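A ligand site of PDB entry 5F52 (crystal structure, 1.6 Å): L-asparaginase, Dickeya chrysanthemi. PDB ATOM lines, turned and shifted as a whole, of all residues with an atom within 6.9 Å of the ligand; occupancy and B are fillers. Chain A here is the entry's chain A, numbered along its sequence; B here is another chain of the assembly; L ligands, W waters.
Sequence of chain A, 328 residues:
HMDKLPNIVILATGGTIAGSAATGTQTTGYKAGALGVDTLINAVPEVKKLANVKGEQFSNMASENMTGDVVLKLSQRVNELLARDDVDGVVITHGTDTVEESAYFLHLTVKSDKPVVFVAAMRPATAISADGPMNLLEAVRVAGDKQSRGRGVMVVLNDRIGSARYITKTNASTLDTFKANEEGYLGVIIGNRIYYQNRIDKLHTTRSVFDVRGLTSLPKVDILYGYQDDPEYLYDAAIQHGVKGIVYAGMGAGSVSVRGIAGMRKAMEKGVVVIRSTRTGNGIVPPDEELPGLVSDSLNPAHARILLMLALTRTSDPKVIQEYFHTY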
ATOM      1  N   GLY A  14      -4.424  16.254  22.830  1.00  0.00           N
ATOM      2  CA  GLY A  14      -4.786  17.026  21.683  1.00  0.00           C
ATOM      3  C   GLY A  14      -5.167  18.475  22.074  1.00  0.00           C
ATOM      4  O   GLY A  14      -4.543  19.072  22.944  1.00  0.00           O
ATOM      5  N   GLY A  15      -6.150  19.038  21.374  1.00  0.00           N
ATOM      6  CA  GLY A  15      -6.600  20.387  21.634  1.00  0.00           C
ATOM      7  C   GLY A  15      -5.905  21.428  20.802  1.00  0.00           C
ATOM      8  O   GLY A  15      -4.902  21.177  20.113  1.00  0.00           O
ATOM      9  N   THR A  16      -6.437  22.640  20.866  1.00  0.00           N
ATOM     10  CA  THR A  16      -5.885  23.774  20.213  1.00  0.00           C
ATOM     11  C   THR A  16      -4.524  24.066  20.715  1.00  0.00           C
ATOM     12  O   THR A  16      -3.674  24.644  19.995  1.00  0.00           O
ATOM     13  CB  THR A  16      -6.825  24.957  20.410  1.00  0.00           C
ATOM     14  OG1 THR A  16      -8.048  24.690  19.703  1.00  0.00           O
ATOM     15  CG2 THR A  16      -6.263  26.311  19.894  1.00  0.00           C
ATOM     16  N   ILE A  17      -4.249  23.710  21.964  1.00  0.00           N
ATOM     17  CA  ILE A  17      -2.881  23.896  22.480  1.00  0.00           C
ATOM     18  C   ILE A  17      -1.831  23.157  21.556  1.00  0.00           C
ATOM     19  O   ILE A  17      -0.677  23.571  21.458  1.00  0.00           O
ATOM     20  CB  ILE A  17      -2.786  23.401  23.935  1.00  0.00           C
ATOM     21  CG1 ILE A  17      -1.442  23.769  24.582  1.00  0.00           C
ATOM     22  CG2 ILE A  17      -3.025  21.890  24.030  1.00  0.00           C
ATOM     23  CD1 ILE A  17      -1.477  23.641  26.083  1.00  0.00           C
ATOM     24  N   ALA A  18      -2.267  22.091  20.938  1.00  0.00           N
ATOM     25  CA  ALA A  18      -1.500  21.290  19.942  1.00  0.00           C
ATOM     26  C   ALA A  18      -1.911  21.562  18.469  1.00  0.00           C
ATOM     27  O   ALA A  18      -1.655  20.750  17.578  1.00  0.00           O
ATOM     28  CB  ALA A  18      -1.639  19.815  20.269  1.00  0.00           C
ATOM     29  N   TYR A  30      -7.558  24.394  10.703  1.00  0.00           N
ATOM     30  CA  TYR A  30      -6.364  23.681  11.205  1.00  0.00           C
ATOM     31  C   TYR A  30      -6.893  22.624  12.143  1.00  0.00           C
ATOM     32  O   TYR A  30      -8.011  22.775  12.665  1.00  0.00           O
ATOM     33  CB  TYR A  30      -5.353  24.625  11.909  1.00  0.00           C
ATOM     34  CG  TYR A  30      -5.875  25.204  13.192  1.00  0.00           C
ATOM     35  CD1 TYR A  30      -5.804  24.463  14.389  1.00  0.00           C
ATOM     36  CD2 TYR A  30      -6.475  26.454  13.229  1.00  0.00           C
ATOM     37  CE1 TYR A  30      -6.318  24.951  15.559  1.00  0.00           C
ATOM     38  CE2 TYR A  30      -6.984  26.954  14.417  1.00  0.00           C
ATOM     39  CZ  TYR A  30      -6.901  26.195  15.569  1.00  0.00           C
ATOM     40  OH  TYR A  30      -7.388  26.628  16.754  1.00  0.00           O
ATOM     41  N   ALA A  32      -7.076  20.831  15.551  1.00  0.00           N
ATOM     42  CA  ALA A  32      -6.777  20.942  16.976  1.00  0.00           C
ATOM     43  C   ALA A  32      -6.309  19.653  17.633  1.00  0.00           C
ATOM     44  O   ALA A  32      -7.098  19.066  18.445  1.00  0.00           O
ATOM     45  CB  ALA A  32      -8.029  21.339  17.715  1.00  0.00           C
ATOM     46  N   GLY A  33      -5.015  19.387  17.613  1.00  0.00           N
ATOM     47  CA  GLY A  33      -4.487  18.084  18.012  1.00  0.00           C
ATOM     48  C   GLY A  33      -3.636  17.528  16.889  1.00  0.00           C
ATOM     49  O   GLY A  33      -3.808  16.387  16.506  1.00  0.00           O
ATOM     50  N   MET A  61      -6.525  14.563  19.613  1.00  0.00           N
ATOM     51  CA  MET A  61      -7.834  14.856  19.037  1.00  0.00           C
ATOM     52  C   MET A  61      -8.344  16.202  19.508  1.00  0.00           C
ATOM     53  O   MET A  61      -7.863  16.729  20.510  1.00  0.00           O
ATOM     54  CB  MET A  61      -8.812  13.761  19.445  1.00  0.00           C
ATOM     55  CG  MET A  61      -9.220  13.781  20.898  1.00  0.00           C
ATOM     56  SD  MET A  61     -10.433  12.498  21.319  1.00  0.00           S
ATOM     57  CE  MET A  61      -9.327  11.078  21.474  1.00  0.00           C
ATOM     58  N   ALA A  62      -9.322  16.729  18.775  1.00  0.00           N
ATOM     59  CA  ALA A  62     -10.073  17.861  19.244  1.00  0.00           C
ATOM     60  C   ALA A  62     -10.952  17.356  20.387  1.00  0.00           C
ATOM     61  O   ALA A  62     -11.520  16.311  20.337  1.00  0.00           O
ATOM     62  CB  ALA A  62     -10.868  18.460  18.104  1.00  0.00           C
ATOM     63  N   SER A  63     -11.090  18.164  21.426  1.00  0.00           N
ATOM     64  CA  SER A  63     -11.793  17.715  22.640  1.00  0.00           C
ATOM     65  C   SER A  63     -13.267  17.587  22.470  1.00  0.00           C
ATOM     66  O   SER A  63     -13.884  16.831  23.226  1.00  0.00           O
ATOM     67  CB  SER A  63     -11.472  18.532  23.888  1.00  0.00           C
ATOM     68  OG  SER A  63     -12.150  19.761  23.921  1.00  0.00           O
ATOM     69  N   GLU A  64     -13.820  18.178  21.443  1.00  0.00           N
ATOM     70  CA  GLU A  64     -15.234  17.902  21.138  1.00  0.00           C
ATOM     71  C   GLU A  64     -15.448  16.435  20.782  1.00  0.00           C
ATOM     72  O   GLU A  64     -16.576  15.961  20.845  1.00  0.00           O
ATOM     73  CB  GLU A  64     -15.765  18.807  20.023  1.00  0.00           C
ATOM     74  CG  GLU A  64     -15.042  18.734  18.682  1.00  0.00           C
ATOM     75  CD  GLU A  64     -13.935  19.736  18.517  1.00  0.00           C
ATOM     76  OE1 GLU A  64     -13.287  20.125  19.561  1.00  0.00           O
ATOM     77  OE2 GLU A  64     -13.733  20.211  17.320  1.00  0.00           O
ATOM     78  N   ASN A  65     -14.383  15.734  20.388  1.00  0.00           N
ATOM     79  CA  ASN A  65     -14.464  14.323  20.098  1.00  0.00           C
ATOM     80  C   ASN A  65     -14.058  13.371  21.188  1.00  0.00           C
ATOM     81  O   ASN A  65     -14.099  12.163  21.033  1.00  0.00           O
ATOM     82  CB  ASN A  65     -13.693  14.038  18.852  1.00  0.00           C
ATOM     83  CG  ASN A  65     -14.482  14.441  17.675  1.00  0.00           C
ATOM     84  OD1 ASN A  65     -15.643  14.035  17.522  1.00  0.00           O
ATOM     85  ND2 ASN A  65     -13.896  15.217  16.817  1.00  0.00           N
ATOM     86  N   HIS A  94      -4.942  19.307  26.755  1.00  0.00           N
ATOM     87  CA  HIS A  94      -6.315  18.917  26.295  1.00  0.00           C
ATOM     88  C   HIS A  94      -6.953  20.059  25.588  1.00  0.00           C
ATOM     89  O   HIS A  94      -6.569  21.236  25.792  1.00  0.00           O
ATOM     90  CB  HIS A  94      -7.095  18.538  27.555  1.00  0.00           C
ATOM     91  CG  HIS A  94      -8.378  17.755  27.391  1.00  0.00           C
ATOM     92  ND1 HIS A  94      -9.570  18.334  27.002  1.00  0.00           N
ATOM     93  CD2 HIS A  94      -8.678  16.475  27.736  1.00  0.00           C
ATOM     94  CE1 HIS A  94     -10.541  17.424  27.038  1.00  0.00           C
ATOM     95  NE2 HIS A  94     -10.052  16.315  27.564  1.00  0.00           N
ATOM     96  N   GLY A  95      -7.959  19.788  24.784  1.00  0.00           N
ATOM     97  CA  GLY A  95      -8.762  20.868  24.205  1.00  0.00           C
ATOM     98  C   GLY A  95      -9.594  21.585  25.274  1.00  0.00           C
ATOM     99  O   GLY A  95      -9.972  20.970  26.286  1.00  0.00           O
ATOM    100  N   THR A  96      -9.885  22.851  25.046  1.00  0.00           N
ATOM    101  CA  THR A  96     -10.678  23.576  26.025  1.00  0.00           C
ATOM    102  C   THR A  96     -12.131  23.155  26.006  1.00  0.00           C
ATOM    103  O   THR A  96     -12.823  23.363  27.011  1.00  0.00           O
ATOM    104  CB  THR A  96     -10.666  25.101  25.744  1.00  0.00           C
ATOM    105  OG1 THR A  96     -11.131  25.359  24.432  1.00  0.00           O
ATOM    106  CG2 THR A  96      -9.254  25.619  25.871  1.00  0.00           C
ATOM    107  N   ASP A  97     -12.643  22.677  24.896  1.00  0.00           N
ATOM    108  CA  ASP A  97     -14.124  22.561  24.784  1.00  0.00           C
ATOM    109  C   ASP A  97     -14.735  21.597  25.805  1.00  0.00           C
ATOM    110  O   ASP A  97     -15.844  21.881  26.308  1.00  0.00           O
ATOM    111  CB  ASP A  97     -14.508  22.137  23.377  1.00  0.00           C
ATOM    112  CG  ASP A  97     -14.294  23.262  22.334  1.00  0.00           C
ATOM    113  OD1 ASP A  97     -14.081  24.433  22.725  1.00  0.00           O
ATOM    114  OD2 ASP A  97     -14.271  22.917  21.145  1.00  0.00           O
ATOM    115  N   THR A  98     -14.061  20.477  26.098  1.00  0.00           N
ATOM    116  CA  THR A  98     -14.582  19.503  27.080  1.00  0.00           C
ATOM    117  C   THR A  98     -13.603  19.211  28.153  1.00  0.00           C
ATOM    118  O   THR A  98     -13.795  18.247  28.884  1.00  0.00           O
ATOM    119  CB  THR A  98     -15.079  18.192  26.397  1.00  0.00           C
ATOM    120  OG1 THR A  98     -13.967  17.447  25.905  1.00  0.00           O
ATOM    121  CG2 THR A  98     -16.045  18.527  25.327  1.00  0.00           C
ATOM    122  N   VAL A  99     -12.601  20.055  28.342  1.00  0.00           N
ATOM    123  CA  VAL A  99     -11.683  19.829  29.443  1.00  0.00           C
ATOM    124  C   VAL A  99     -12.404  19.728  30.783  1.00  0.00           C
ATOM    125  O   VAL A  99     -11.961  18.990  31.664  1.00  0.00           O
ATOM    126  CB  VAL A  99     -10.530  20.862  29.484  1.00  0.00           C
ATOM    127  CG1 VAL A  99     -10.991  22.223  29.895  1.00  0.00           C
ATOM    128  CG2 VAL A  99      -9.417  20.360  30.403  1.00  0.00           C
ATOM    129  N   ALA A 120      -4.735  23.810  28.788  1.00  0.00           N
ATOM    130  CA  ALA A 120      -5.291  23.986  27.463  1.00  0.00           C
ATOM    131  C   ALA A 120      -4.959  25.346  26.959  1.00  0.00           C
ATOM    132  O   ALA A 120      -4.266  26.113  27.654  1.00  0.00           O
ATOM    133  CB  ALA A 120      -6.786  23.755  27.479  1.00  0.00           C
ATOM    134  N   ALA A 121      -5.360  25.650  25.758  1.00  0.00           N
ATOM    135  CA  ALA A 121      -5.065  26.951  25.149  1.00  0.00           C
ATOM    136  C   ALA A 121      -6.225  27.342  24.218  1.00  0.00           C
ATOM    137  O   ALA A 121      -6.756  26.511  23.536  1.00  0.00           O
ATOM    138  CB  ALA A 121      -3.791  26.924  24.318  1.00  0.00           C
ATOM    139  N   MET A 122      -6.581  28.614  24.239  1.00  0.00           N
ATOM    140  CA  MET A 122      -7.570  29.149  23.348  1.00  0.00           C
ATOM    141  C   MET A 122      -7.076  29.524  21.981  1.00  0.00           C
ATOM    142  O   MET A 122      -7.868  29.536  21.036  1.00  0.00           O
ATOM    143  CB  MET A 122      -8.328  30.266  24.005  1.00  0.00           C
ATOM    144  CG  MET A 122      -9.138  29.812  25.217  1.00  0.00           C
ATOM    145  SD  MET A 122     -10.597  28.856  24.688  1.00  0.00           S
ATOM    146  CE  MET A 122     -11.600  30.128  23.980  1.00  0.00           C
ATOM    147  N   ARG A 123      -5.785  29.736  21.832  1.00  0.00           N
ATOM    148  CA  ARG A 123      -5.149  30.056  20.525  1.00  0.00           C
ATOM    149  C   ARG A 123      -4.186  28.934  20.183  1.00  0.00           C
ATOM    150  O   ARG A 123      -3.505  28.356  21.088  1.00  0.00           O
ATOM    151  CB  ARG A 123      -4.359  31.323  20.614  1.00  0.00           C
ATOM    152  CG  ARG A 123      -5.211  32.585  20.907  1.00  0.00           C
ATOM    153  CD  ARG A 123      -4.357  33.799  21.119  1.00  0.00           C
ATOM    154  NE  ARG A 123      -5.217  34.950  21.374  1.00  0.00           N
ATOM    155  CZ  ARG A 123      -4.834  36.080  21.950  1.00  0.00           C
ATOM    156  NH1 ARG A 123      -3.590  36.226  22.377  1.00  0.00           N
ATOM    157  NH2 ARG A 123      -5.726  37.061  22.188  1.00  0.00           N
ATOM    158  N   LYS A 169     -15.878  26.454  31.135  1.00  0.00           N
ATOM    159  CA  LYS A 169     -15.599  27.335  30.041  1.00  0.00           C
ATOM    160  C   LYS A 169     -16.831  28.225  29.908  1.00  0.00           C
ATOM    161  O   LYS A 169     -17.935  27.773  29.587  1.00  0.00           O
ATOM    162  CB  LYS A 169     -15.346  26.529  28.757  1.00  0.00           C
ATOM    163  CG  LYS A 169     -14.936  27.366  27.575  1.00  0.00           C
ATOM    164  CD  LYS A 169     -14.505  26.513  26.354  1.00  0.00           C
ATOM    165  CE  LYS A 169     -14.097  27.462  25.250  1.00  0.00           C
ATOM    166  NZ  LYS A 169     -13.512  26.745  24.099  1.00  0.00           N
ATOM    167  N   ALA A 172     -17.271  31.352  24.740  1.00  0.00           N
ATOM    168  CA  ALA A 172     -16.913  30.583  23.595  1.00  0.00           C
ATOM    169  C   ALA A 172     -15.506  30.780  23.060  1.00  0.00           C
ATOM    170  O   ALA A 172     -14.924  29.903  22.555  1.00  0.00           O
ATOM    171  CB  ALA A 172     -17.892  30.882  22.459  1.00  0.00           C
ATOM    172  N   MET B 251     -20.395  22.686  22.364  1.00  0.00           N
ATOM    173  CA  MET B 251     -19.179  22.709  23.146  1.00  0.00           C
ATOM    174  C   MET B 251     -18.349  23.934  22.661  1.00  0.00           C
ATOM    175  O   MET B 251     -18.131  24.137  21.475  1.00  0.00           O
ATOM    176  CB  MET B 251     -18.416  21.391  22.948  1.00  0.00           C
ATOM    177  CG  MET B 251     -19.216  20.212  23.479  1.00  0.00           C
ATOM    178  SD  MET B 251     -18.541  18.606  22.963  1.00  0.00           S
ATOM    179  CE  MET B 251     -19.365  18.402  21.402  1.00  0.00           C
ATOM    180  N   GLY B 252     -17.875  24.747  23.577  1.00  0.00           N
ATOM    181  CA  GLY B 252     -17.032  25.852  23.172  1.00  0.00           C
ATOM    182  C   GLY B 252     -17.664  26.739  22.131  1.00  0.00           C
ATOM    183  O   GLY B 252     -18.845  27.102  22.268  1.00  0.00           O
ATOM    184  N   ALA B 253     -16.890  27.076  21.106  1.00  0.00           N
ATOM    185  CA  ALA B 253     -17.349  27.970  20.044  1.00  0.00           C
ATOM    186  C   ALA B 253     -18.133  27.215  18.973  1.00  0.00           C
ATOM    187  O   ALA B 253     -17.765  27.198  17.855  1.00  0.00           O
ATOM    188  CB  ALA B 253     -16.172  28.717  19.491  1.00  0.00           C
ATOM    189  N   SER B 255     -18.399  24.081  18.647  1.00  0.00           N
ATOM    190  CA  SER B 255     -17.681  22.908  18.153  1.00  0.00           C
ATOM    191  C   SER B 255     -18.574  21.698  18.152  1.00  0.00           C
ATOM    192  O   SER B 255     -19.437  21.536  19.013  1.00  0.00           O
ATOM    193  CB  SER B 255     -16.460  22.573  18.985  1.00  0.00           C
ATOM    194  OG  SER B 255     -15.682  23.667  18.946  1.00  0.00           O
HETATM  195  N1  LIG L   1     -11.934  22.632  19.727  1.00  0.00           N
HETATM  196  C1  LIG L   1     -10.658  22.879  20.476  1.00  0.00           C
HETATM  197  C2  LIG L   1     -10.665  21.674  21.408  1.00  0.00           C
HETATM  198  O1  LIG L   1     -11.466  21.647  22.391  1.00  0.00           O
HETATM  199  C3  LIG L   1     -10.752  24.250  21.157  1.00  0.00           C
HETATM  200  C4  LIG L   1      -9.575  24.586  22.070  1.00  0.00           C
HETATM  201  O2  LIG L   1      -9.540  25.845  22.389  1.00  0.00           O
HETATM  202  O3  LIG L   1      -8.794  23.625  22.464  1.00  0.00           O
HETATM  203  O4  LIG L   1      -9.976  20.668  21.141  1.00  0.00           O
HETATM  204  O   HOH W   1      -6.350  23.407  24.079  1.00  0.00           O
HETATM  205  O   HOH W   2     -11.568  21.405  16.570  1.00  0.00           O
HETATM  206  O   HOH W   3     -11.584  24.445  17.657  1.00  0.00           O
HETATM  207  O   HOH W   4     -10.149  27.789  20.957  1.00  0.00           O
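The backbone NH (N) of Ser 63 is in hydrogen-bond range of an oxygen (O4) of the ligand (2.8 Å).
O1 of the ligand sits at hydrogen-bond distance from OG of Ser 63 (2.5 Å).
An oxygen (O3) of the ligand sits at hydrogen-bond distance from the backbone NH (N) of Thr 96, at 2.9 Å.
The side-chain hydroxyl of Thr 96 lies within hydrogen-bond range of an oxygen (O2) of the ligand, 2.6 Å away.
The backbone NH (N) of Asp 97 is in hydrogen-bond range of an oxygen (O1) of the ligand (3.0 Å).
The side-chain carboxylate (OD2) of Asp 97 lies within salt-bridge range of a nitrogen (N1) of the ligand, 2.7 Å away.
An oxygen (O3) of the ligand is in hydrogen-bond range of the backbone NH of Thr 16, at 3.0 Å.
The side-chain hydroxyl of Thr 16 sits close to an oxygen (O3) of the ligand.
The side-chain carboxylate (OE1) of Glu 64 is in salt-bridge range of a nitrogen (N1) of the ligand (2.9 Å).
The backbone carbonyl oxygen of Ala 121 lies close to an oxygen (O2) of the ligand (3.1 Å).
The backbone NH (N) of Asp 97 sits at hydrogen-bond distance from the side-chain hydroxyl (OG) of Ser 63.
The side-chain hydroxyl of Thr 96 is in hydrogen-bond range of the side-chain sulfur of Met 122, at 3.5 Å.
NZ of Lys 169 sits at hydrogen-bond distance from OG1 of Thr 96.
The side-chain hydroxyl (OG) of Ser 255 of chain B lies within hydrogen-bond range of the side-chain carboxylate (OD2) of Asp 97 (2.7 Å).
NZ of Lys 169 lies within salt-bridge range of OD1 of Asp 97 (2.7 Å).
The backbone carbonyl oxygen (O) of Ala 32 is in hydrogen-bond range of the backbone NH (N) of Ala 62 (3.2 Å).
The backbone NH (N) of Gly 15 sits at hydrogen-bond distance from the backbone carbonyl oxygen (O) of Ala 32.
The backbone NH (N) of Gly 33 lies within hydrogen-bond range of the backbone carbonyl oxygen (O) of Gly 15, 3.1 Å away.
Gly 15 touches the ligand (CA to O4, 3.4 Å).
Ala 32 touches the ligand (CB to O4, 3.997 Å).
Ala 62 touches the ligand.
CA of Gly 95 touches O3 of the ligand, at 3.3 Å.
Met 122 touches the ligand (SD to O2, 3.9 Å).
Ser 255 of chain B touches the ligand.
Hydrophobic or aromatic side chains within 4 Å of the ligand: Ala 32, Ala 62 and Met 122.
Water W4 lies within hydrogen-bond range of an oxygen (O2) of the ligand (2.5 Å) and the backbone carbonyl oxygen of Met 122 (2.9 Å).
Water W2 lies within hydrogen-bond range of OE2 of Glu 64 and N1 of the ligand.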
